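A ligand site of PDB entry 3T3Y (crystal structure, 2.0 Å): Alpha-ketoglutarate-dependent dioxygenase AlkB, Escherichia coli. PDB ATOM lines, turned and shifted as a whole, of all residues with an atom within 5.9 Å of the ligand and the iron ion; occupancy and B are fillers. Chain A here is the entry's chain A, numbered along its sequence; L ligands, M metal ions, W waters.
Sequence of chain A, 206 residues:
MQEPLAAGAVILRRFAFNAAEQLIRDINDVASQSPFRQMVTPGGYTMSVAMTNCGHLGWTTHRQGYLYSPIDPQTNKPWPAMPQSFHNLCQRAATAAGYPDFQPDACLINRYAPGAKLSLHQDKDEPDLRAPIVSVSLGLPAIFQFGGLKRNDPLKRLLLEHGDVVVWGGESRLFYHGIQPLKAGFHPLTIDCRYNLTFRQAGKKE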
ATOM      1  N   ASN A 110       7.779 -14.276   3.236  1.00  0.00           N
ATOM      2  CA  ASN A 110       8.619 -15.466   3.258  1.00  0.00           C
ATOM      3  C   ASN A 110      10.091 -15.057   3.314  1.00  0.00           C
ATOM      4  O   ASN A 110      10.488 -14.131   2.637  1.00  0.00           O
ATOM      5  CB  ASN A 110       8.430 -16.287   1.969  1.00  0.00           C
ATOM      6  CG  ASN A 110       7.116 -17.055   1.935  1.00  0.00           C
ATOM      7  OD1 ASN A 110       6.360 -17.019   2.891  1.00  0.00           O
ATOM      8  ND2 ASN A 110       6.854 -17.752   0.824  1.00  0.00           N
ATOM      9  N   TYR A 112      13.946 -16.833   2.809  1.00  0.00           N
ATOM     10  CA  TYR A 112      14.660 -18.022   2.374  1.00  0.00           C
ATOM     11  C   TYR A 112      16.138 -17.891   2.660  1.00  0.00           C
ATOM     12  O   TYR A 112      16.786 -16.994   2.129  1.00  0.00           O
ATOM     13  CB  TYR A 112      14.526 -18.217   0.843  1.00  0.00           C
ATOM     14  CG  TYR A 112      13.121 -18.469   0.370  1.00  0.00           C
ATOM     15  CD1 TYR A 112      12.205 -17.427   0.282  1.00  0.00           C
ATOM     16  CD2 TYR A 112      12.713 -19.741   0.000  1.00  0.00           C
ATOM     17  CE1 TYR A 112      10.910 -17.651  -0.159  1.00  0.00           C
ATOM     18  CE2 TYR A 112      11.430 -19.981  -0.445  1.00  0.00           C
ATOM     19  CZ  TYR A 112      10.536 -18.925  -0.515  1.00  0.00           C
ATOM     20  OH  TYR A 112       9.251 -19.171  -0.941  1.00  0.00           O
ATOM     21  N   LEU A 118      10.246 -23.856  -1.325  1.00  0.00           N
ATOM     22  CA  LEU A 118       8.829 -23.889  -1.015  1.00  0.00           C
ATOM     23  C   LEU A 118       8.168 -24.970  -1.871  1.00  0.00           C
ATOM     24  O   LEU A 118       8.209 -24.924  -3.106  1.00  0.00           O
ATOM     25  CB  LEU A 118       8.191 -22.514  -1.272  1.00  0.00           C
ATOM     26  CG  LEU A 118       6.713 -22.361  -0.912  1.00  0.00           C
ATOM     27  CD1 LEU A 118       6.523 -22.407   0.612  1.00  0.00           C
ATOM     28  CD2 LEU A 118       6.156 -21.061  -1.478  1.00  0.00           C
ATOM     29  N   HIS A 121       2.390 -26.158  -4.387  1.00  0.00           N
ATOM     30  CA  HIS A 121       1.144 -25.895  -3.702  1.00  0.00           C
ATOM     31  C   HIS A 121       0.269 -24.956  -4.523  1.00  0.00           C
ATOM     32  O   HIS A 121       0.726 -24.323  -5.474  1.00  0.00           O
ATOM     33  CB  HIS A 121       1.441 -25.234  -2.355  1.00  0.00           C
ATOM     34  CG  HIS A 121       1.919 -23.821  -2.492  1.00  0.00           C
ATOM     35  ND1 HIS A 121       3.244 -23.507  -2.704  1.00  0.00           N
ATOM     36  CD2 HIS A 121       1.253 -22.646  -2.467  1.00  0.00           C
ATOM     37  CE1 HIS A 121       3.375 -22.194  -2.807  1.00  0.00           C
ATOM     38  NE2 HIS A 121       2.180 -21.652  -2.672  1.00  0.00           N
ATOM     39  N   GLN A 122      -1.008 -24.882  -4.142  1.00  0.00           N
ATOM     40  CA  GLN A 122      -1.930 -23.898  -4.692  1.00  0.00           C
ATOM     41  C   GLN A 122      -2.293 -22.929  -3.589  1.00  0.00           C
ATOM     42  O   GLN A 122      -2.359 -23.303  -2.417  1.00  0.00           O
ATOM     43  CB  GLN A 122      -3.220 -24.566  -5.155  1.00  0.00           C
ATOM     44  CG  GLN A 122      -3.093 -25.731  -6.093  1.00  0.00           C
ATOM     45  CD  GLN A 122      -4.449 -26.366  -6.353  1.00  0.00           C
ATOM     46  OE1 GLN A 122      -4.954 -27.137  -5.535  1.00  0.00           O
ATOM     47  NE2 GLN A 122      -5.064 -26.020  -7.486  1.00  0.00           N
ATOM     48  N   ASP A 123      -2.533 -21.672  -3.942  1.00  0.00           N
ATOM     49  CA  ASP A 123      -3.185 -20.746  -3.024  1.00  0.00           C
ATOM     50  C   ASP A 123      -4.680 -20.720  -3.326  1.00  0.00           C
ATOM     51  O   ASP A 123      -5.138 -19.983  -4.204  1.00  0.00           O
ATOM     52  CB  ASP A 123      -2.563 -19.360  -3.110  1.00  0.00           C
ATOM     53  CG  ASP A 123      -1.137 -19.330  -2.609  1.00  0.00           C
ATOM     54  OD1 ASP A 123      -0.240 -19.637  -3.411  1.00  0.00           O
ATOM     55  OD2 ASP A 123      -0.913 -19.027  -1.424  1.00  0.00           O
ATOM     56  N   ILE A 133      -3.052 -12.551  -6.822  1.00  0.00           N
ATOM     57  CA  ILE A 133      -2.077 -12.408  -5.748  1.00  0.00           C
ATOM     58  C   ILE A 133      -0.932 -11.610  -6.336  1.00  0.00           C
ATOM     59  O   ILE A 133      -0.511 -11.854  -7.480  1.00  0.00           O
ATOM     60  CB  ILE A 133      -1.630 -13.777  -5.205  1.00  0.00           C
ATOM     61  CG1 ILE A 133      -2.764 -14.405  -4.405  1.00  0.00           C
ATOM     62  CG2 ILE A 133      -0.374 -13.656  -4.315  1.00  0.00           C
ATOM     63  CD1 ILE A 133      -2.432 -15.776  -3.855  1.00  0.00           C
ATOM     64  N   VAL A 134      -0.451 -10.626  -5.573  1.00  0.00           N
ATOM     65  CA  VAL A 134       0.690  -9.830  -5.994  1.00  0.00           C
ATOM     66  C   VAL A 134       1.929 -10.297  -5.247  1.00  0.00           C
ATOM     67  O   VAL A 134       1.960 -10.340  -4.003  1.00  0.00           O
ATOM     68  CB  VAL A 134       0.463  -8.317  -5.760  1.00  0.00           C
ATOM     69  CG1 VAL A 134       1.697  -7.507  -6.144  1.00  0.00           C
ATOM     70  CG2 VAL A 134      -0.765  -7.835  -6.532  1.00  0.00           C
ATOM     71  N   SER A 135       2.957 -10.663  -6.011  1.00  0.00           N
ATOM     72  CA  SER A 135       4.136 -11.282  -5.444  1.00  0.00           C
ATOM     73  C   SER A 135       5.405 -10.496  -5.769  1.00  0.00           C
ATOM     74  O   SER A 135       5.709 -10.206  -6.940  1.00  0.00           O
ATOM     75  CB  SER A 135       4.256 -12.717  -5.941  1.00  0.00           C
ATOM     76  OG  SER A 135       5.497 -13.286  -5.552  1.00  0.00           O
ATOM     77  N   SER A 137       9.595 -10.089  -5.198  1.00  0.00           N
ATOM     78  CA  SER A 137      10.863 -10.748  -4.887  1.00  0.00           C
ATOM     79  C   SER A 137      11.927  -9.734  -4.521  1.00  0.00           C
ATOM     80  O   SER A 137      12.061  -8.696  -5.183  1.00  0.00           O
ATOM     81  CB  SER A 137      11.339 -11.583  -6.082  1.00  0.00           C
ATOM     82  OG  SER A 137      10.518 -12.715  -6.277  1.00  0.00           O
ATOM     83  N   PHE A 144      11.394 -20.018  -9.797  1.00  0.00           N
ATOM     84  CA  PHE A 144       9.979 -20.206  -9.545  1.00  0.00           C
ATOM     85  C   PHE A 144       9.482 -21.258 -10.531  1.00  0.00           C
ATOM     86  O   PHE A 144       9.755 -21.180 -11.729  1.00  0.00           O
ATOM     87  CB  PHE A 144       9.262 -18.854  -9.745  1.00  0.00           C
ATOM     88  CG  PHE A 144       7.772 -18.903  -9.565  1.00  0.00           C
ATOM     89  CD1 PHE A 144       7.207 -18.849  -8.307  1.00  0.00           C
ATOM     90  CD2 PHE A 144       6.943 -18.951 -10.667  1.00  0.00           C
ATOM     91  CE1 PHE A 144       5.831 -18.867  -8.156  1.00  0.00           C
ATOM     92  CE2 PHE A 144       5.575 -18.973 -10.527  1.00  0.00           C
ATOM     93  CZ  PHE A 144       5.015 -18.930  -9.261  1.00  0.00           C
ATOM     94  N   LEU A 160      13.217 -15.668 -10.792  1.00  0.00           N
ATOM     95  CA  LEU A 160      12.760 -14.391 -10.247  1.00  0.00           C
ATOM     96  C   LEU A 160      13.925 -13.691  -9.556  1.00  0.00           C
ATOM     97  O   LEU A 160      14.639 -14.280  -8.730  1.00  0.00           O
ATOM     98  CB  LEU A 160      11.615 -14.584  -9.239  1.00  0.00           C
ATOM     99  CG  LEU A 160      10.305 -15.166  -9.751  1.00  0.00           C
ATOM    100  CD1 LEU A 160       9.317 -15.343  -8.604  1.00  0.00           C
ATOM    101  CD2 LEU A 160       9.707 -14.271 -10.849  1.00  0.00           C
ATOM    102  N   VAL A 166       5.404 -10.289  -9.709  1.00  0.00           N
ATOM    103  CA  VAL A 166       4.500 -11.077 -10.533  1.00  0.00           C
ATOM    104  C   VAL A 166       3.088 -10.810 -10.045  1.00  0.00           C
ATOM    105  O   VAL A 166       2.818 -10.871  -8.852  1.00  0.00           O
ATOM    106  CB  VAL A 166       4.804 -12.572 -10.394  1.00  0.00           C
ATOM    107  CG1 VAL A 166       3.774 -13.407 -11.164  1.00  0.00           C
ATOM    108  CG2 VAL A 166       6.247 -12.878 -10.891  1.00  0.00           C
ATOM    109  N   TRP A 168      -0.291 -12.506 -10.186  1.00  0.00           N
ATOM    110  CA  TRP A 168      -0.719 -13.868 -10.459  1.00  0.00           C
ATOM    111  C   TRP A 168      -2.245 -13.880 -10.514  1.00  0.00           C
ATOM    112  O   TRP A 168      -2.908 -13.908  -9.472  1.00  0.00           O
ATOM    113  CB  TRP A 168      -0.217 -14.746  -9.305  1.00  0.00           C
ATOM    114  CG  TRP A 168      -0.302 -16.242  -9.443  1.00  0.00           C
ATOM    115  CD1 TRP A 168      -1.139 -17.089  -8.760  1.00  0.00           C
ATOM    116  CD2 TRP A 168       0.527 -17.088 -10.263  1.00  0.00           C
ATOM    117  NE1 TRP A 168      -0.901 -18.397  -9.119  1.00  0.00           N
ATOM    118  CE2 TRP A 168       0.119 -18.426 -10.042  1.00  0.00           C
ATOM    119  CE3 TRP A 168       1.565 -16.848 -11.164  1.00  0.00           C
ATOM    120  CZ2 TRP A 168       0.697 -19.518 -10.694  1.00  0.00           C
ATOM    121  CZ3 TRP A 168       2.151 -17.936 -11.814  1.00  0.00           C
ATOM    122  CH2 TRP A 168       1.717 -19.245 -11.576  1.00  0.00           C
ATOM    123  N   ARG A 173      -4.170 -18.322 -11.699  1.00  0.00           N
ATOM    124  CA  ARG A 173      -4.480 -18.088 -10.292  1.00  0.00           C
ATOM    125  C   ARG A 173      -4.427 -19.367  -9.451  1.00  0.00           C
ATOM    126  O   ARG A 173      -3.828 -19.379  -8.374  1.00  0.00           O
ATOM    127  CB  ARG A 173      -5.846 -17.399 -10.152  1.00  0.00           C
ATOM    128  CG  ARG A 173      -6.263 -17.097  -8.726  1.00  0.00           C
ATOM    129  CD  ARG A 173      -5.282 -16.178  -7.989  1.00  0.00           C
ATOM    130  NE  ARG A 173      -5.743 -16.003  -6.618  1.00  0.00           N
ATOM    131  CZ  ARG A 173      -5.537 -16.894  -5.649  1.00  0.00           C
ATOM    132  NH1 ARG A 173      -4.842 -17.991  -5.921  1.00  0.00           N
ATOM    133  NH2 ARG A 173      -6.005 -16.691  -4.429  1.00  0.00           N
ATOM    134  N   HIS A 177       2.392 -24.278  -7.827  1.00  0.00           N
ATOM    135  CA  HIS A 177       3.661 -23.573  -8.019  1.00  0.00           C
ATOM    136  C   HIS A 177       4.526 -23.693  -6.786  1.00  0.00           C
ATOM    137  O   HIS A 177       4.056 -24.080  -5.707  1.00  0.00           O
ATOM    138  CB  HIS A 177       3.415 -22.088  -8.312  1.00  0.00           C
ATOM    139  CG  HIS A 177       2.589 -21.405  -7.268  1.00  0.00           C
ATOM    140  ND1 HIS A 177       1.216 -21.500  -7.225  1.00  0.00           N
ATOM    141  CD2 HIS A 177       2.948 -20.650  -6.191  1.00  0.00           C
ATOM    142  CE1 HIS A 177       0.762 -20.821  -6.182  1.00  0.00           C
ATOM    143  NE2 HIS A 177       1.784 -20.286  -5.549  1.00  0.00           N
ATOM    144  N   ILE A 179       8.981 -22.980  -5.193  1.00  0.00           N
ATOM    145  CA  ILE A 179      10.301 -22.379  -5.316  1.00  0.00           C
ATOM    146  C   ILE A 179      11.361 -23.454  -5.095  1.00  0.00           C
ATOM    147  O   ILE A 179      11.300 -24.208  -4.115  1.00  0.00           O
ATOM    148  CB  ILE A 179      10.468 -21.221  -4.293  1.00  0.00           C
ATOM    149  CG1 ILE A 179       9.513 -20.068  -4.614  1.00  0.00           C
ATOM    150  CG2 ILE A 179      11.909 -20.700  -4.269  1.00  0.00           C
ATOM    151  CD1 ILE A 179       9.972 -19.184  -5.761  1.00  0.00           C
ATOM    152  N   ARG A 194      16.611 -14.394   0.484  1.00  0.00           N
ATOM    153  CA  ARG A 194      15.631 -13.853  -0.431  1.00  0.00           C
ATOM    154  C   ARG A 194      14.368 -13.634   0.397  1.00  0.00           C
ATOM    155  O   ARG A 194      14.026 -14.450   1.241  1.00  0.00           O
ATOM    156  CB  ARG A 194      15.333 -14.835  -1.551  1.00  0.00           C
ATOM    157  CG  ARG A 194      14.107 -14.456  -2.376  1.00  0.00           C
ATOM    158  CD  ARG A 194      13.875 -15.468  -3.477  1.00  0.00           C
ATOM    159  NE  ARG A 194      12.743 -15.090  -4.313  1.00  0.00           N
ATOM    160  CZ  ARG A 194      11.510 -15.576  -4.164  1.00  0.00           C
ATOM    161  NH1 ARG A 194      11.262 -16.502  -3.249  1.00  0.00           N
ATOM    162  NH2 ARG A 194      10.532 -15.160  -4.971  1.00  0.00           N
ATOM    163  N   ASN A 196      10.186 -12.811  -0.043  1.00  0.00           N
ATOM    164  CA  ASN A 196       9.065 -12.717  -0.956  1.00  0.00           C
ATOM    165  C   ASN A 196       7.843 -12.186  -0.227  1.00  0.00           C
ATOM    166  O   ASN A 196       7.533 -12.635   0.883  1.00  0.00           O
ATOM    167  CB  ASN A 196       8.778 -14.076  -1.613  1.00  0.00           C
ATOM    168  CG  ASN A 196       7.501 -14.063  -2.421  1.00  0.00           C
ATOM    169  OD1 ASN A 196       6.486 -14.595  -1.988  1.00  0.00           O
ATOM    170  ND2 ASN A 196       7.543 -13.484  -3.616  1.00  0.00           N
ATOM    171  N   THR A 198       3.741 -11.809  -0.639  1.00  0.00           N
ATOM    172  CA  THR A 198       2.541 -12.118  -1.412  1.00  0.00           C
ATOM    173  C   THR A 198       1.335 -11.434  -0.791  1.00  0.00           C
ATOM    174  O   THR A 198       0.932 -11.740   0.331  1.00  0.00           O
ATOM    175  CB  THR A 198       2.254 -13.644  -1.604  1.00  0.00           C
ATOM    176  OG1 THR A 198       2.449 -14.344  -0.366  1.00  0.00           O
ATOM    177  CG2 THR A 198       3.145 -14.244  -2.677  1.00  0.00           C
ATOM    178  N   ARG A 200      -2.640 -10.469  -0.668  1.00  0.00           N
ATOM    179  CA  ARG A 200      -3.879 -11.203  -0.882  1.00  0.00           C
ATOM    180  C   ARG A 200      -5.103 -10.455  -0.381  1.00  0.00           C
ATOM    181  O   ARG A 200      -5.033  -9.711   0.597  1.00  0.00           O
ATOM    182  CB  ARG A 200      -3.823 -12.559  -0.149  1.00  0.00           C
ATOM    183  CG  ARG A 200      -2.575 -13.393  -0.464  1.00  0.00           C
ATOM    184  CD  ARG A 200      -1.862 -13.836   0.809  1.00  0.00           C
ATOM    185  NE  ARG A 200      -0.622 -14.567   0.525  1.00  0.00           N
ATOM    186  CZ  ARG A 200      -0.599 -15.795   0.030  1.00  0.00           C
ATOM    187  NH1 ARG A 200      -1.727 -16.442  -0.240  1.00  0.00           N
ATOM    188  NH2 ARG A 200       0.567 -16.388  -0.209  1.00  0.00           N
HETATM  189  C1  LIG L   1       7.870 -17.148  -3.454  1.00  0.00           C
HETATM  190  N1  LIG L   1       5.565 -17.260  -4.083  1.00  0.00           N
HETATM  191  O1  LIG L   1       8.094 -16.460  -4.552  1.00  0.00           O
HETATM  192  C2  LIG L   1       6.540 -17.834  -3.274  1.00  0.00           C
HETATM  193  N2  LIG L   1       1.958 -17.693  -4.743  1.00  0.00           N
HETATM  194  O2  LIG L   1       8.712 -17.199  -2.561  1.00  0.00           O
HETATM  195  C3  LIG L   1       4.253 -17.822  -4.105  1.00  0.00           C
HETATM  196  O3  LIG L   1       4.019 -18.786  -3.378  1.00  0.00           O
HETATM  197  C4  LIG L   1       3.202 -17.241  -4.931  1.00  0.00           C
HETATM  198  O4  LIG L   1       4.801 -15.869  -6.036  1.00  0.00           O
HETATM  199  C5  LIG L   1       0.944 -17.185  -5.451  1.00  0.00           C
HETATM  200  C6  LIG L   1       1.180 -16.221  -6.409  1.00  0.00           C
HETATM  201  C7  LIG L   1       2.487 -15.750  -6.637  1.00  0.00           C
HETATM  202  C8  LIG L   1       3.516 -16.272  -5.868  1.00  0.00           C
HETATM  203 FE    FE M   1       1.889 -19.507  -3.429  1.00  0.00          FE
HETATM  204  O   HOH W   1       1.761 -18.633  -1.349  1.00  0.00           O
HETATM  205  O   HOH W   2       5.442 -15.479  -8.454  1.00  0.00           O
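Three residues have an atom within 4 Å of the iron ion: His 121, Asp 123 and His 177.
Along chain A the residues within 4 Å of the iron ion span positions 121 to 177.
The nearest printed residue that does not touch the iron ion is Arg 200 (4.7 Å).
Water W1 lies within hydrogen-bond range of OD2 of Asp 123 (2.7 Å) and NH2 of Arg 200 (2.8 Å).
Residues that only touch the ligand: Asn 110 (3.9 Å), Leu 118 (3.7 Å), Ile 133 (3.7 Å), Phe 144 (3.8 Å), Trp 168 (3.4 Å), Ile 179 (3.5 Å) and Thr 198 (3.8 Å).
Of the 21 residues printed, 14 come within 4 Å of the ligand.
The side-chain amide nitrogen of Asn 110 sits at hydrogen-bond distance from the side-chain hydroxyl of Tyr 112.
ND2 of Asn 196 is in hydrogen-bond range of OG of Ser 135, at 2.8 Å.
NH2 of Arg 194 is in hydrogen-bond range of OG of Ser 137, 2.8 Å away.
O of Asn 196 sits at hydrogen-bond distance from N of Asn 110 (2.9 Å).
The backbone carbonyl oxygen of Leu 118 is in hydrogen-bond range of the backbone NH of Ile 179 (3.0 Å).
The guanidinium group (NH2) of Arg 200 lies within hydrogen-bond range of the side-chain hydroxyl (OG1) of Thr 198 (2.8 Å).
O of Ile 133 sits at hydrogen-bond distance from N of Trp 168 (2.8 Å).
The indole nitrogen (NE1) of Trp 168 is in hydrogen-bond range of the backbone carbonyl oxygen (O) of Arg 173 (3.2 Å).
OD1 of Asp 123 binds the iron ion.
N2 of the ligand is bound to the iron ion (2.2 Å).
O3 of the ligand binds the iron ion (2.2 Å).
The iron ion is bound by water W1, 2.3 Å away.
NE2 of His 177 is bound to the iron ion, 2.3 Å away.
The iron ion is bound by NE2 of His 121 (2.3 Å).
The side-chain hydroxyl (OG) of Ser 135 sits at hydrogen-bond distance from an oxygen (O4) of the ligand (2.7 Å).
The guanidinium group (NH1) of Arg 194 lies within salt-bridge range of an oxygen (O2) of the ligand, 2.7 Å away.
O2 of the ligand lies within hydrogen-bond range of OH of Tyr 112 (2.6 Å).
An oxygen (O1) of the ligand is in hydrogen-bond range of the side-chain amide nitrogen (ND2) of Asn 196 (3.2 Å).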
